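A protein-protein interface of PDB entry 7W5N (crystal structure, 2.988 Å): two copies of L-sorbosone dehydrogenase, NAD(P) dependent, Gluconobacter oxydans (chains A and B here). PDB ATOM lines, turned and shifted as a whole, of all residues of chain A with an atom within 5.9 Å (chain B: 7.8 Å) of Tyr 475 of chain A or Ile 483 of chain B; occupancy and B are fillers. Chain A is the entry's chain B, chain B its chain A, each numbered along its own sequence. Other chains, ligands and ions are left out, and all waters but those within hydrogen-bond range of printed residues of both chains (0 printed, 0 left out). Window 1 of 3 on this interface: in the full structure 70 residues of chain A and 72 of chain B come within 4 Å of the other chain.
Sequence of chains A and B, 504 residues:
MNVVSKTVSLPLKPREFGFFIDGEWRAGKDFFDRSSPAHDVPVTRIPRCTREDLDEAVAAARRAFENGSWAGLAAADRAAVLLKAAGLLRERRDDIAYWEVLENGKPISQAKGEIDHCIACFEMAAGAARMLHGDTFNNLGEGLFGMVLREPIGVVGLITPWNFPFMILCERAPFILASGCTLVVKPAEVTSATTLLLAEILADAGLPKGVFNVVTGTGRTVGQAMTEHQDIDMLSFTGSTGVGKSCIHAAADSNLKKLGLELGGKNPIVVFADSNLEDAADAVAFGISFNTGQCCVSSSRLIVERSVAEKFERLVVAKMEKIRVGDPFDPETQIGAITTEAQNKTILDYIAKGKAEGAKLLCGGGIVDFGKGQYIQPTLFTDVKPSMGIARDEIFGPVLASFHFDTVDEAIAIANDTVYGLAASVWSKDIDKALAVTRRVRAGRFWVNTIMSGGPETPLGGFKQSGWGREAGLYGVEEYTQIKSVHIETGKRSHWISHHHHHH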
ATOM      1  N   ALA A 443     -24.727   1.496  15.429  1.00  0.00           N
ATOM      2  CA  ALA A 443     -23.517   1.916  14.684  1.00  0.00           C
ATOM      3  C   ALA A 443     -23.907   3.051  13.746  1.00  0.00           C
ATOM      4  O   ALA A 443     -25.065   3.058  13.308  1.00  0.00           O
ATOM      5  CB  ALA A 443     -22.934   0.756  13.921  1.00  0.00           C
ATOM      6  N   GLY A 444     -22.987   3.969  13.462  1.00  0.00           N
ATOM      7  CA  GLY A 444     -23.292   5.201  12.709  1.00  0.00           C
ATOM      8  C   GLY A 444     -23.016   5.045  11.229  1.00  0.00           C
ATOM      9  O   GLY A 444     -23.465   5.914  10.451  1.00  0.00           O
ATOM     10  N   ARG A 445     -22.273   4.006  10.852  1.00  0.00           N
ATOM     11  CA  ARG A 445     -21.855   3.784   9.445  1.00  0.00           C
ATOM     12  C   ARG A 445     -22.216   2.364   9.001  1.00  0.00           C
ATOM     13  O   ARG A 445     -21.474   1.405   9.351  1.00  0.00           O
ATOM     14  CB  ARG A 445     -20.352   4.014   9.291  1.00  0.00           C
ATOM     15  CG  ARG A 445     -19.821   5.236  10.023  1.00  0.00           C
ATOM     16  CD  ARG A 445     -18.442   5.622   9.549  1.00  0.00           C
ATOM     17  NE  ARG A 445     -18.450   5.788   8.104  1.00  0.00           N
ATOM     18  CZ  ARG A 445     -17.382   6.048   7.363  1.00  0.00           C
ATOM     19  NH1 ARG A 445     -16.188   6.177   7.925  1.00  0.00           N
ATOM     20  NH2 ARG A 445     -17.538   6.172   6.054  1.00  0.00           N
ATOM     21  N   GLU A 457     -21.071  12.838   0.196  1.00  0.00           N
ATOM     22  CA  GLU A 457     -22.503  13.242   0.158  1.00  0.00           C
ATOM     23  C   GLU A 457     -23.129  13.040   1.550  1.00  0.00           C
ATOM     24  O   GLU A 457     -24.009  13.851   1.935  1.00  0.00           O
ATOM     25  CB  GLU A 457     -23.261  12.448  -0.920  1.00  0.00           C
ATOM     26  CG  GLU A 457     -22.737  12.668  -2.342  1.00  0.00           C
ATOM     27  CD  GLU A 457     -21.577  11.798  -2.829  1.00  0.00           C
ATOM     28  OE1 GLU A 457     -21.344  10.729  -2.233  1.00  0.00           O
ATOM     29  OE2 GLU A 457     -20.900  12.185  -3.808  1.00  0.00           O
ATOM     30  N   THR A 458     -22.713  11.994   2.272  1.00  0.00           N
ATOM     31  CA  THR A 458     -23.399  11.476   3.484  1.00  0.00           C
ATOM     32  C   THR A 458     -22.473  11.651   4.671  1.00  0.00           C
ATOM     33  O   THR A 458     -21.265  11.604   4.501  1.00  0.00           O
ATOM     34  CB  THR A 458     -23.776   9.998   3.334  1.00  0.00           C
ATOM     35  OG1 THR A 458     -22.597   9.281   2.960  1.00  0.00           O
ATOM     36  CG2 THR A 458     -24.880   9.778   2.322  1.00  0.00           C
ATOM     37  N   PRO A 459     -23.010  11.843   5.896  1.00  0.00           N
ATOM     38  CA  PRO A 459     -22.174  11.896   7.096  1.00  0.00           C
ATOM     39  C   PRO A 459     -21.567  10.546   7.513  1.00  0.00           C
ATOM     40  O   PRO A 459     -21.933   9.519   6.996  1.00  0.00           O
ATOM     41  CB  PRO A 459     -23.128  12.435   8.175  1.00  0.00           C
ATOM     42  CG  PRO A 459     -24.523  12.044   7.690  1.00  0.00           C
ATOM     43  CD  PRO A 459     -24.437  12.075   6.179  1.00  0.00           C
ATOM     44  N   GLY A 461     -19.731   8.842  11.372  1.00  0.00           N
ATOM     45  CA  GLY A 461     -19.305   8.893  12.778  1.00  0.00           C
ATOM     46  C   GLY A 461     -19.879   7.725  13.561  1.00  0.00           C
ATOM     47  O   GLY A 461     -20.457   6.817  12.945  1.00  0.00           O
ATOM     48  N   PHE A 463     -21.616   5.692  17.233  1.00  0.00           N
ATOM     49  CA  PHE A 463     -22.425   5.571  18.459  1.00  0.00           C
ATOM     50  C   PHE A 463     -21.501   5.301  19.646  1.00  0.00           C
ATOM     51  O   PHE A 463     -20.285   5.088  19.518  1.00  0.00           O
ATOM     52  CB  PHE A 463     -23.423   4.423  18.319  1.00  0.00           C
ATOM     53  CG  PHE A 463     -24.617   4.694  17.435  1.00  0.00           C
ATOM     54  CD1 PHE A 463     -24.467   5.260  16.169  1.00  0.00           C
ATOM     55  CD2 PHE A 463     -25.890   4.329  17.855  1.00  0.00           C
ATOM     56  CE1 PHE A 463     -25.566   5.451  15.349  1.00  0.00           C
ATOM     57  CE2 PHE A 463     -26.984   4.523  17.030  1.00  0.00           C
ATOM     58  CZ  PHE A 463     -26.819   5.070  15.778  1.00  0.00           C
ATOM     59  N   ARG A 470     -20.494  14.215  13.745  1.00  0.00           N
ATOM     60  CA  ARG A 470     -20.456  13.550  12.420  1.00  0.00           C
ATOM     61  C   ARG A 470     -19.576  14.379  11.471  1.00  0.00           C
ATOM     62  O   ARG A 470     -19.587  15.616  11.587  1.00  0.00           O
ATOM     63  CB  ARG A 470     -21.886  13.378  11.902  1.00  0.00           C
ATOM     64  CG  ARG A 470     -22.757  12.456  12.748  1.00  0.00           C
ATOM     65  CD  ARG A 470     -22.159  11.066  12.829  1.00  0.00           C
ATOM     66  NE  ARG A 470     -23.092  10.006  13.195  1.00  0.00           N
ATOM     67  CZ  ARG A 470     -23.028   9.292  14.315  1.00  0.00           C
ATOM     68  NH1 ARG A 470     -22.085   9.520  15.205  1.00  0.00           N
ATOM     69  NH2 ARG A 470     -23.898   8.332  14.552  1.00  0.00           N
ATOM     70  N   GLU A 471     -18.823  13.735  10.575  1.00  0.00           N
ATOM     71  CA  GLU A 471     -17.929  14.437   9.615  1.00  0.00           C
ATOM     72  C   GLU A 471     -18.444  14.210   8.197  1.00  0.00           C
ATOM     73  O   GLU A 471     -19.119  13.191   8.010  1.00  0.00           O
ATOM     74  CB  GLU A 471     -16.510  13.906   9.758  1.00  0.00           C
ATOM     75  CG  GLU A 471     -16.003  13.973  11.174  1.00  0.00           C
ATOM     76  CD  GLU A 471     -15.639  15.357  11.680  1.00  0.00           C
ATOM     77  OE1 GLU A 471     -15.905  16.347  10.947  1.00  0.00           O
ATOM     78  OE2 GLU A 471     -15.062  15.429  12.818  1.00  0.00           O
ATOM     79  N   ALA A 472     -18.138  15.120   7.263  1.00  0.00           N
ATOM     80  CA  ALA A 472     -18.481  15.020   5.821  1.00  0.00           C
ATOM     81  C   ALA A 472     -19.972  15.280   5.591  1.00  0.00           C
ATOM     82  O   ALA A 472     -20.722  15.360   6.570  1.00  0.00           O
ATOM     83  CB  ALA A 472     -18.117  13.658   5.273  1.00  0.00           C
ATOM     84  N   GLY A 473     -20.395  15.342   4.328  1.00  0.00           N
ATOM     85  CA  GLY A 473     -21.776  15.715   3.957  1.00  0.00           C
ATOM     86  C   GLY A 473     -22.045  17.149   4.357  1.00  0.00           C
ATOM     87  O   GLY A 473     -21.108  17.819   4.827  1.00  0.00           O
ATOM     88  N   LEU A 474     -23.273  17.618   4.216  1.00  0.00           N
ATOM     89  CA  LEU A 474     -23.623  18.941   4.777  1.00  0.00           C
ATOM     90  C   LEU A 474     -23.550  18.898   6.322  1.00  0.00           C
ATOM     91  O   LEU A 474     -23.287  19.964   6.907  1.00  0.00           O
ATOM     92  CB  LEU A 474     -25.003  19.323   4.242  1.00  0.00           C
ATOM     93  CG  LEU A 474     -25.596  20.658   4.694  1.00  0.00           C
ATOM     94  CD1 LEU A 474     -24.546  21.750   4.790  1.00  0.00           C
ATOM     95  CD2 LEU A 474     -26.694  21.078   3.734  1.00  0.00           C
ATOM     96  N   TYR A 475     -23.732  17.742   6.986  1.00  0.00           N
ATOM     97  CA  TYR A 475     -23.720  17.646   8.476  1.00  0.00           C
ATOM     98  C   TYR A 475     -22.325  18.008   9.010  1.00  0.00           C
ATOM     99  O   TYR A 475     -22.209  18.552  10.109  1.00  0.00           O
ATOM    100  CB  TYR A 475     -24.037  16.245   9.008  1.00  0.00           C
ATOM    101  CG  TYR A 475     -25.386  15.674   8.673  1.00  0.00           C
ATOM    102  CD1 TYR A 475     -25.688  15.246   7.390  1.00  0.00           C
ATOM    103  CD2 TYR A 475     -26.353  15.512   9.648  1.00  0.00           C
ATOM    104  CE1 TYR A 475     -26.926  14.701   7.072  1.00  0.00           C
ATOM    105  CE2 TYR A 475     -27.601  14.967   9.350  1.00  0.00           C
ATOM    106  CZ  TYR A 475     -27.889  14.550   8.059  1.00  0.00           C
ATOM    107  OH  TYR A 475     -29.105  14.006   7.755  1.00  0.00           O
ATOM    108  N   GLY A 476     -21.277  17.682   8.269  1.00  0.00           N
ATOM    109  CA  GLY A 476     -19.888  17.860   8.735  1.00  0.00           C
ATOM    110  C   GLY A 476     -19.430  19.295   8.595  1.00  0.00           C
ATOM    111  O   GLY A 476     -18.679  19.770   9.443  1.00  0.00           O
ATOM    112  N   VAL A 477     -19.866  19.969   7.547  1.00  0.00           N
ATOM    113  CA  VAL A 477     -19.673  21.437   7.456  1.00  0.00           C
ATOM    114  C   VAL A 477     -20.289  22.074   8.710  1.00  0.00           C
ATOM    115  O   VAL A 477     -19.597  22.934   9.314  1.00  0.00           O
ATOM    116  CB  VAL A 477     -20.251  22.004   6.142  1.00  0.00           C
ATOM    117  CG1 VAL A 477     -20.437  23.519   6.205  1.00  0.00           C
ATOM    118  CG2 VAL A 477     -19.387  21.621   4.942  1.00  0.00           C
ATOM    119  N   GLU A 478     -21.499  21.629   9.079  1.00  0.00           N
ATOM    120  CA  GLU A 478     -22.405  22.244  10.085  1.00  0.00           C
ATOM    121  C   GLU A 478     -21.831  22.056  11.497  1.00  0.00           C
ATOM    122  O   GLU A 478     -21.997  22.933  12.368  1.00  0.00           O
ATOM    123  CB  GLU A 478     -23.791  21.597   9.997  1.00  0.00           C
ATOM    124  CG  GLU A 478     -24.678  22.066   8.852  1.00  0.00           C
ATOM    125  CD  GLU A 478     -26.047  21.395   8.843  1.00  0.00           C
ATOM    126  OE1 GLU A 478     -26.262  20.494   9.697  1.00  0.00           O
ATOM    127  OE2 GLU A 478     -26.906  21.771   7.989  1.00  0.00           O
ATOM    128  N   GLU A 479     -21.182  20.926  11.722  1.00  0.00           N
ATOM    129  CA  GLU A 479     -20.558  20.602  13.024  1.00  0.00           C
ATOM    130  C   GLU A 479     -19.680  21.768  13.476  1.00  0.00           C
ATOM    131  O   GLU A 479     -19.519  21.909  14.678  1.00  0.00           O
ATOM    132  CB  GLU A 479     -19.679  19.359  12.930  1.00  0.00           C
ATOM    133  CG  GLU A 479     -20.463  18.128  12.581  1.00  0.00           C
ATOM    134  CD  GLU A 479     -21.528  17.740  13.594  1.00  0.00           C
ATOM    135  OE1 GLU A 479     -21.149  17.126  14.635  1.00  0.00           O
ATOM    136  OE2 GLU A 479     -22.731  18.018  13.326  1.00  0.00           O
ATOM    137  N   TYR A 480     -19.060  22.510  12.562  1.00  0.00           N
ATOM    138  CA  TYR A 480     -18.008  23.493  12.931  1.00  0.00           C
ATOM    139  C   TYR A 480     -18.595  24.893  12.790  1.00  0.00           C
ATOM    140  O   TYR A 480     -17.845  25.913  12.739  1.00  0.00           O
ATOM    141  CB  TYR A 480     -16.727  23.266  12.128  1.00  0.00           C
ATOM    142  CG  TYR A 480     -16.149  21.888  12.297  1.00  0.00           C
ATOM    143  CD1 TYR A 480     -16.671  20.812  11.604  1.00  0.00           C
ATOM    144  CD2 TYR A 480     -15.102  21.653  13.162  1.00  0.00           C
ATOM    145  CE1 TYR A 480     -16.160  19.533  11.750  1.00  0.00           C
ATOM    146  CE2 TYR A 480     -14.578  20.382  13.328  1.00  0.00           C
ATOM    147  CZ  TYR A 480     -15.104  19.317  12.615  1.00  0.00           C
ATOM    148  OH  TYR A 480     -14.580  18.067  12.773  1.00  0.00           O
ATOM    149  N   HIS B 133     -36.856  13.294  10.945  1.00  0.00           N
ATOM    150  CA  HIS B 133     -36.554  12.694   9.620  1.00  0.00           C
ATOM    151  C   HIS B 133     -35.049  12.711   9.345  1.00  0.00           C
ATOM    152  O   HIS B 133     -34.396  13.637   9.766  1.00  0.00           O
ATOM    153  CB  HIS B 133     -37.366  13.431   8.531  1.00  0.00           C
ATOM    154  CG  HIS B 133     -36.870  14.800   8.173  1.00  0.00           C
ATOM    155  ND1 HIS B 133     -36.833  15.847   9.075  1.00  0.00           N
ATOM    156  CD2 HIS B 133     -36.401  15.303   7.009  1.00  0.00           C
ATOM    157  CE1 HIS B 133     -36.352  16.934   8.492  1.00  0.00           C
ATOM    158  NE2 HIS B 133     -36.081  16.625   7.220  1.00  0.00           N
ATOM    159  N   GLY B 134     -34.543  11.717   8.637  1.00  0.00           N
ATOM    160  CA  GLY B 134     -33.201  11.767   8.035  1.00  0.00           C
ATOM    161  C   GLY B 134     -33.298  12.002   6.539  1.00  0.00           C
ATOM    162  O   GLY B 134     -34.272  12.661   6.137  1.00  0.00           O
ATOM    163  N   ASP B 135     -32.380  11.452   5.738  1.00  0.00           N
ATOM    164  CA  ASP B 135     -32.190  11.851   4.322  1.00  0.00           C
ATOM    165  C   ASP B 135     -32.127  10.608   3.436  1.00  0.00           C
ATOM    166  O   ASP B 135     -31.571   9.587   3.903  1.00  0.00           O
ATOM    167  CB  ASP B 135     -30.870  12.596   4.096  1.00  0.00           C
ATOM    168  CG  ASP B 135     -30.704  13.928   4.805  1.00  0.00           C
ATOM    169  OD1 ASP B 135     -31.736  14.626   4.974  1.00  0.00           O
ATOM    170  OD2 ASP B 135     -29.528  14.261   5.166  1.00  0.00           O
ATOM    171  N   THR B 136     -32.593  10.716   2.186  1.00  0.00           N
ATOM    172  CA  THR B 136     -32.359   9.702   1.131  1.00  0.00           C
ATOM    173  C   THR B 136     -31.436  10.283   0.063  1.00  0.00           C
ATOM    174  O   THR B 136     -31.512  11.469  -0.214  1.00  0.00           O
ATOM    175  CB  THR B 136     -33.650   9.226   0.468  1.00  0.00           C
ATOM    176  OG1 THR B 136     -34.067  10.273  -0.412  1.00  0.00           O
ATOM    177  CG2 THR B 136     -34.705   8.848   1.485  1.00  0.00           C
ATOM    178  N   PHE B 137     -30.611   9.425  -0.519  1.00  0.00           N
ATOM    179  CA  PHE B 137     -29.652   9.778  -1.583  1.00  0.00           C
ATOM    180  C   PHE B 137     -29.863   8.821  -2.754  1.00  0.00           C
ATOM    181  O   PHE B 137     -29.183   7.797  -2.919  1.00  0.00           O
ATOM    182  CB  PHE B 137     -28.245   9.794  -0.997  1.00  0.00           C
ATOM    183  CG  PHE B 137     -27.968  11.029  -0.188  1.00  0.00           C
ATOM    184  CD1 PHE B 137     -27.740  12.244  -0.817  1.00  0.00           C
ATOM    185  CD2 PHE B 137     -27.923  10.960   1.192  1.00  0.00           C
ATOM    186  CE1 PHE B 137     -27.438  13.372  -0.073  1.00  0.00           C
ATOM    187  CE2 PHE B 137     -27.633  12.090   1.938  1.00  0.00           C
ATOM    188  CZ  PHE B 137     -27.386  13.293   1.305  1.00  0.00           C
ATOM    189  N   MET B 147     -28.743   6.604   2.275  1.00  0.00           N
ATOM    190  CA  MET B 147     -29.808   6.788   3.282  1.00  0.00           C
ATOM    191  C   MET B 147     -29.153   7.307   4.571  1.00  0.00           C
ATOM    192  O   MET B 147     -28.043   6.818   4.906  1.00  0.00           O
ATOM    193  CB  MET B 147     -30.476   5.429   3.508  1.00  0.00           C
ATOM    194  CG  MET B 147     -31.771   5.500   4.258  1.00  0.00           C
ATOM    195  SD  MET B 147     -32.851   4.158   3.776  1.00  0.00           S
ATOM    196  CE  MET B 147     -32.152   2.809   4.727  1.00  0.00           C
ATOM    197  N   VAL B 148     -29.751   8.298   5.232  1.00  0.00           N
ATOM    198  CA  VAL B 148     -29.326   8.707   6.602  1.00  0.00           C
ATOM    199  C   VAL B 148     -30.540   8.593   7.519  1.00  0.00           C
ATOM    200  O   VAL B 148     -31.513   9.264   7.247  1.00  0.00           O
ATOM    201  CB  VAL B 148     -28.689  10.110   6.646  1.00  0.00           C
ATOM    202  CG1 VAL B 148     -28.431  10.581   8.074  1.00  0.00           C
ATOM    203  CG2 VAL B 148     -27.407  10.169   5.831  1.00  0.00           C
ATOM    204  N   LEU B 149     -30.458   7.709   8.510  1.00  0.00           N
ATOM    205  CA  LEU B 149     -31.518   7.458   9.516  1.00  0.00           C
ATOM    206  C   LEU B 149     -31.232   8.338  10.723  1.00  0.00           C
ATOM    207  O   LEU B 149     -30.073   8.730  10.923  1.00  0.00           O
ATOM    208  CB  LEU B 149     -31.547   5.973   9.921  1.00  0.00           C
ATOM    209  CG  LEU B 149     -31.914   4.978   8.807  1.00  0.00           C
ATOM    210  CD1 LEU B 149     -32.236   3.588   9.357  1.00  0.00           C
ATOM    211  CD2 LEU B 149     -33.086   5.477   7.968  1.00  0.00           C
ATOM    212  N   ARG B 150     -32.277   8.655  11.470  1.00  0.00           N
ATOM    213  CA  ARG B 150     -32.159   9.154  12.858  1.00  0.00           C
ATOM    214  C   ARG B 150     -32.785   8.114  13.796  1.00  0.00           C
ATOM    215  O   ARG B 150     -33.795   7.465  13.425  1.00  0.00           O
ATOM    216  CB  ARG B 150     -32.829  10.520  12.968  1.00  0.00           C
ATOM    217  CG  ARG B 150     -32.029  11.651  12.359  1.00  0.00           C
ATOM    218  CD  ARG B 150     -32.471  12.911  13.031  1.00  0.00           C
ATOM    219  NE  ARG B 150     -31.839  14.038  12.399  1.00  0.00           N
ATOM    220  CZ  ARG B 150     -30.671  14.567  12.748  1.00  0.00           C
ATOM    221  NH1 ARG B 150     -29.966  14.069  13.753  1.00  0.00           N
ATOM    222  NH2 ARG B 150     -30.220  15.617  12.080  1.00  0.00           N
ATOM    223  N   GLU B 151     -32.202   7.924  14.969  1.00  0.00           N
ATOM    224  CA  GLU B 151     -32.850   7.045  15.961  1.00  0.00           C
ATOM    225  C   GLU B 151     -32.633   7.610  17.356  1.00  0.00           C
ATOM    226  O   GLU B 151     -31.701   8.365  17.597  1.00  0.00           O
ATOM    227  CB  GLU B 151     -32.337   5.620  15.806  1.00  0.00           C
ATOM    228  CG  GLU B 151     -30.834   5.507  15.655  1.00  0.00           C
ATOM    229  CD  GLU B 151     -30.406   4.056  15.517  1.00  0.00           C
ATOM    230  OE1 GLU B 151     -30.336   3.367  16.565  1.00  0.00           O
ATOM    231  OE2 GLU B 151     -30.194   3.604  14.357  1.00  0.00           O
ATOM    232  N   GLU B 478     -33.556  16.431  17.836  1.00  0.00           N
ATOM    233  CA  GLU B 478     -32.435  15.835  17.060  1.00  0.00           C
ATOM    234  C   GLU B 478     -31.145  15.713  17.874  1.00  0.00           C
ATOM    235  O   GLU B 478     -30.317  14.881  17.487  1.00  0.00           O
ATOM    236  CB  GLU B 478     -32.129  16.722  15.852  1.00  0.00           C
ATOM    237  CG  GLU B 478     -33.234  16.734  14.805  1.00  0.00           C
ATOM    238  CD  GLU B 478     -32.955  17.719  13.698  1.00  0.00           C
ATOM    239  OE1 GLU B 478     -32.271  18.709  13.982  1.00  0.00           O
ATOM    240  OE2 GLU B 478     -33.403  17.476  12.568  1.00  0.00           O
ATOM    241  N   TYR B 480     -30.659  14.483  20.713  1.00  0.00           N
ATOM    242  CA  TYR B 480     -30.776  13.209  21.467  1.00  0.00           C
ATOM    243  C   TYR B 480     -31.031  12.046  20.506  1.00  0.00           C
ATOM    244  O   TYR B 480     -31.433  10.951  20.943  1.00  0.00           O
ATOM    245  CB  TYR B 480     -31.897  13.371  22.497  1.00  0.00           C
ATOM    246  CG  TYR B 480     -31.631  14.489  23.466  1.00  0.00           C
ATOM    247  CD1 TYR B 480     -30.855  14.281  24.591  1.00  0.00           C
ATOM    248  CD2 TYR B 480     -32.082  15.766  23.227  1.00  0.00           C
ATOM    249  CE1 TYR B 480     -30.588  15.296  25.495  1.00  0.00           C
ATOM    250  CE2 TYR B 480     -31.803  16.801  24.106  1.00  0.00           C
ATOM    251  CZ  TYR B 480     -31.058  16.569  25.253  1.00  0.00           C
ATOM    252  OH  TYR B 480     -30.771  17.570  26.142  1.00  0.00           O
ATOM    253  N   THR B 481     -30.824  12.292  19.217  1.00  0.00           N
ATOM    254  CA  THR B 481     -30.809  11.255  18.152  1.00  0.00           C
ATOM    255  C   THR B 481     -29.362  11.037  17.692  1.00  0.00           C
ATOM    256  O   THR B 481     -28.505  11.938  17.898  1.00  0.00           O
ATOM    257  CB  THR B 481     -31.696  11.598  16.946  1.00  0.00           C
ATOM    258  OG1 THR B 481     -30.983  12.554  16.157  1.00  0.00           O
ATOM    259  CG2 THR B 481     -33.077  12.091  17.331  1.00  0.00           C
ATOM    260  N   GLN B 482     -29.124   9.840  17.149  1.00  0.00           N
ATOM    261  CA  GLN B 482     -27.870   9.406  16.494  1.00  0.00           C
ATOM    262  C   GLN B 482     -28.164   9.277  15.002  1.00  0.00           C
ATOM    263  O   GLN B 482     -29.124   8.569  14.641  1.00  0.00           O
ATOM    264  CB  GLN B 482     -27.361   8.074  17.060  1.00  0.00           C
ATOM    265  CG  GLN B 482     -26.613   8.192  18.381  1.00  0.00           C
ATOM    266  CD  GLN B 482     -25.310   8.955  18.283  1.00  0.00           C
ATOM    267  OE1 GLN B 482     -25.039   9.651  17.302  1.00  0.00           O
ATOM    268  NE2 GLN B 482     -24.490   8.841  19.316  1.00  0.00           N
ATOM    269  N   ILE B 483     -27.381   9.977  14.194  1.00  0.00           N
ATOM    270  CA  ILE B 483     -27.375   9.891  12.711  1.00  0.00           C
ATOM    271  C   ILE B 483     -26.717   8.562  12.332  1.00  0.00           C
ATOM    272  O   ILE B 483     -25.579   8.343  12.750  1.00  0.00           O
ATOM    273  CB  ILE B 483     -26.624  11.119  12.145  1.00  0.00           C
ATOM    274  CG1 ILE B 483     -27.490  12.375  12.233  1.00  0.00           C
ATOM    275  CG2 ILE B 483     -26.119  10.889  10.730  1.00  0.00           C
ATOM    276  CD1 ILE B 483     -26.699  13.639  12.451  1.00  0.00           C
ATOM    277  N   LYS B 484     -27.405   7.735  11.545  1.00  0.00           N
ATOM    278  CA  LYS B 484     -26.895   6.449  10.988  1.00  0.00           C
ATOM    279  C   LYS B 484     -26.846   6.529   9.445  1.00  0.00           C
ATOM    280  O   LYS B 484     -27.914   6.650   8.823  1.00  0.00           O
ATOM    281  CB  LYS B 484     -27.775   5.313  11.527  1.00  0.00           C
ATOM    282  CG  LYS B 484     -27.642   3.975  10.812  1.00  0.00           C
ATOM    283  CD  LYS B 484     -28.532   2.920  11.414  1.00  0.00           C
ATOM    284  CE  LYS B 484     -27.948   2.360  12.693  1.00  0.00           C
ATOM    285  NZ  LYS B 484     -28.958   1.639  13.507  1.00  0.00           N
ATOM    286  N   SER B 485     -25.650   6.476   8.843  1.00  0.00           N
ATOM    287  CA  SER B 485     -25.454   6.397   7.370  1.00  0.00           C
ATOM    288  C   SER B 485     -25.672   4.947   6.912  1.00  0.00           C
ATOM    289  O   SER B 485     -25.027   4.025   7.497  1.00  0.00           O
ATOM    290  CB  SER B 485     -24.084   6.888   6.937  1.00  0.00           C
ATOM    291  OG  SER B 485     -23.814   8.181   7.442  1.00  0.00           O
ATOM    292  N   VAL B 486     -26.538   4.739   5.916  1.00  0.00           N
ATOM    293  CA  VAL B 486     -26.738   3.407   5.281  1.00  0.00           C
ATOM    294  C   VAL B 486     -26.448   3.538   3.784  1.00  0.00           C
ATOM    295  O   VAL B 486     -26.954   4.483   3.151  1.00  0.00           O
ATOM    296  CB  VAL B 486     -28.142   2.851   5.576  1.00  0.00           C
ATOM    297  CG1 VAL B 486     -28.353   1.448   5.018  1.00  0.00           C
ATOM    298  CG2 VAL B 486     -28.416   2.856   7.070  1.00  0.00           C
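The side-chain hydroxyl of Tyr 475 of chain A sits at hydrogen-bond distance from the side-chain carboxylate of Asp 135 of chain B, at 2.6 Å.
The guanidinium group (NH2) of Arg 470 of chain A is in hydrogen-bond range of the side-chain amide oxygen (OE1) of Gln 482 of chain B, at 3.3 Å.
O of Ile 483 of chain B lies within hydrogen-bond range of NH2 of Arg 470 of chain A, 2.5 Å away.
The backbone carbonyl oxygen of Gly 444 of chain A sits at hydrogen-bond distance from the backbone NH of Ser 485 of chain B, 2.8 Å away.
The side-chain hydroxyl (OG) of Ser 485 of chain B lies close to the backbone carbonyl oxygen (O) of Pro 459 of chain A, at 2.4 Å.
2 positions are printed for both chains.
Of the 19 pairs that touch across the chains among the printed residues, none has its exchanged pair printed and touching as well.
Of chain B, only Asp 135 (2.6 Å), Val 148 (3.5 Å), Arg 150 (3.8 Å) and Ile 483 (3.4 Å) come within 4 Å of Tyr 475 of chain A.
Of chain A, only Gly 444, Pro 459, Phe 463, Arg 470 and Tyr 475 come within 4 Å of Ile 483 of chain B.
Of the printed residues of chain A, Asp 135 of chain B touches Tyr 475.
Printed residues of chain B within 4 Å of Glu 457 of chain A: Phe 137.
Printed residues of chain B within 4 Å of Arg 470 of chain A: Gln 482 and Ile 483.
Printed residues of chain A within 4 Å of Ser 485 of chain B: Gly 444 (2.8 Å), Arg 445 (3.6 Å) and Pro 459 (2.4 Å).
Gly 461 of chain A touches none of the printed residues of chain B.
Tyr 480 of chain B touches none of the printed residues of chain A.
The nearest residue of chain B that does not touch Tyr 475 of chain A is Gly 134 of chain B (4.7 Å).
The nearest printed residue of chain A that does not touch Ile 483 of chain B is Ala 443 of chain A (5.3 Å).
The nearest printed residue of chain A that does not touch Lys 484 of chain B is Phe 463 of chain A (4.3 Å).
O of Lys 484 of chain B is in hydrogen-bond range of N of Leu 149 of chain B (2.8 Å).
The guanidinium group (NH2) of Arg 150 of chain B is in salt-bridge range of the side-chain carboxylate (OE2) of Glu 478 of chain B, 3.7 Å away.
The side-chain hydroxyl (OG1) of Thr 481 of chain B sits at hydrogen-bond distance from the guanidinium group (NH1) of Arg 150 of chain B.
N of Arg 470 of chain A lies within hydrogen-bond range of OE1 of Glu 479 of chain A (3.1 Å).
Gly 444 of chain A touches Ile 483 of chain B.
Lys 484 of chain B touches Gly 444 of chain A.
CZ of Phe 137 of chain B touches O of Glu 457 of chain A, 3.5 Å away.
Val 148 of chain B touches Pro 459 of chain A.
Pro 459 of chain A touches Ile 483 of chain B.
Gln 482 of chain B touches Phe 463 of chain A.
Ile 483 of chain B touches Phe 463 of chain A.
Val 148 of chain B touches Tyr 475 of chain A.
Arg 150 of chain B touches Tyr 475 of chain A (NH2 to CE2, 3.8 Å).
Ile 483 of chain B touches Tyr 475 of chain A.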
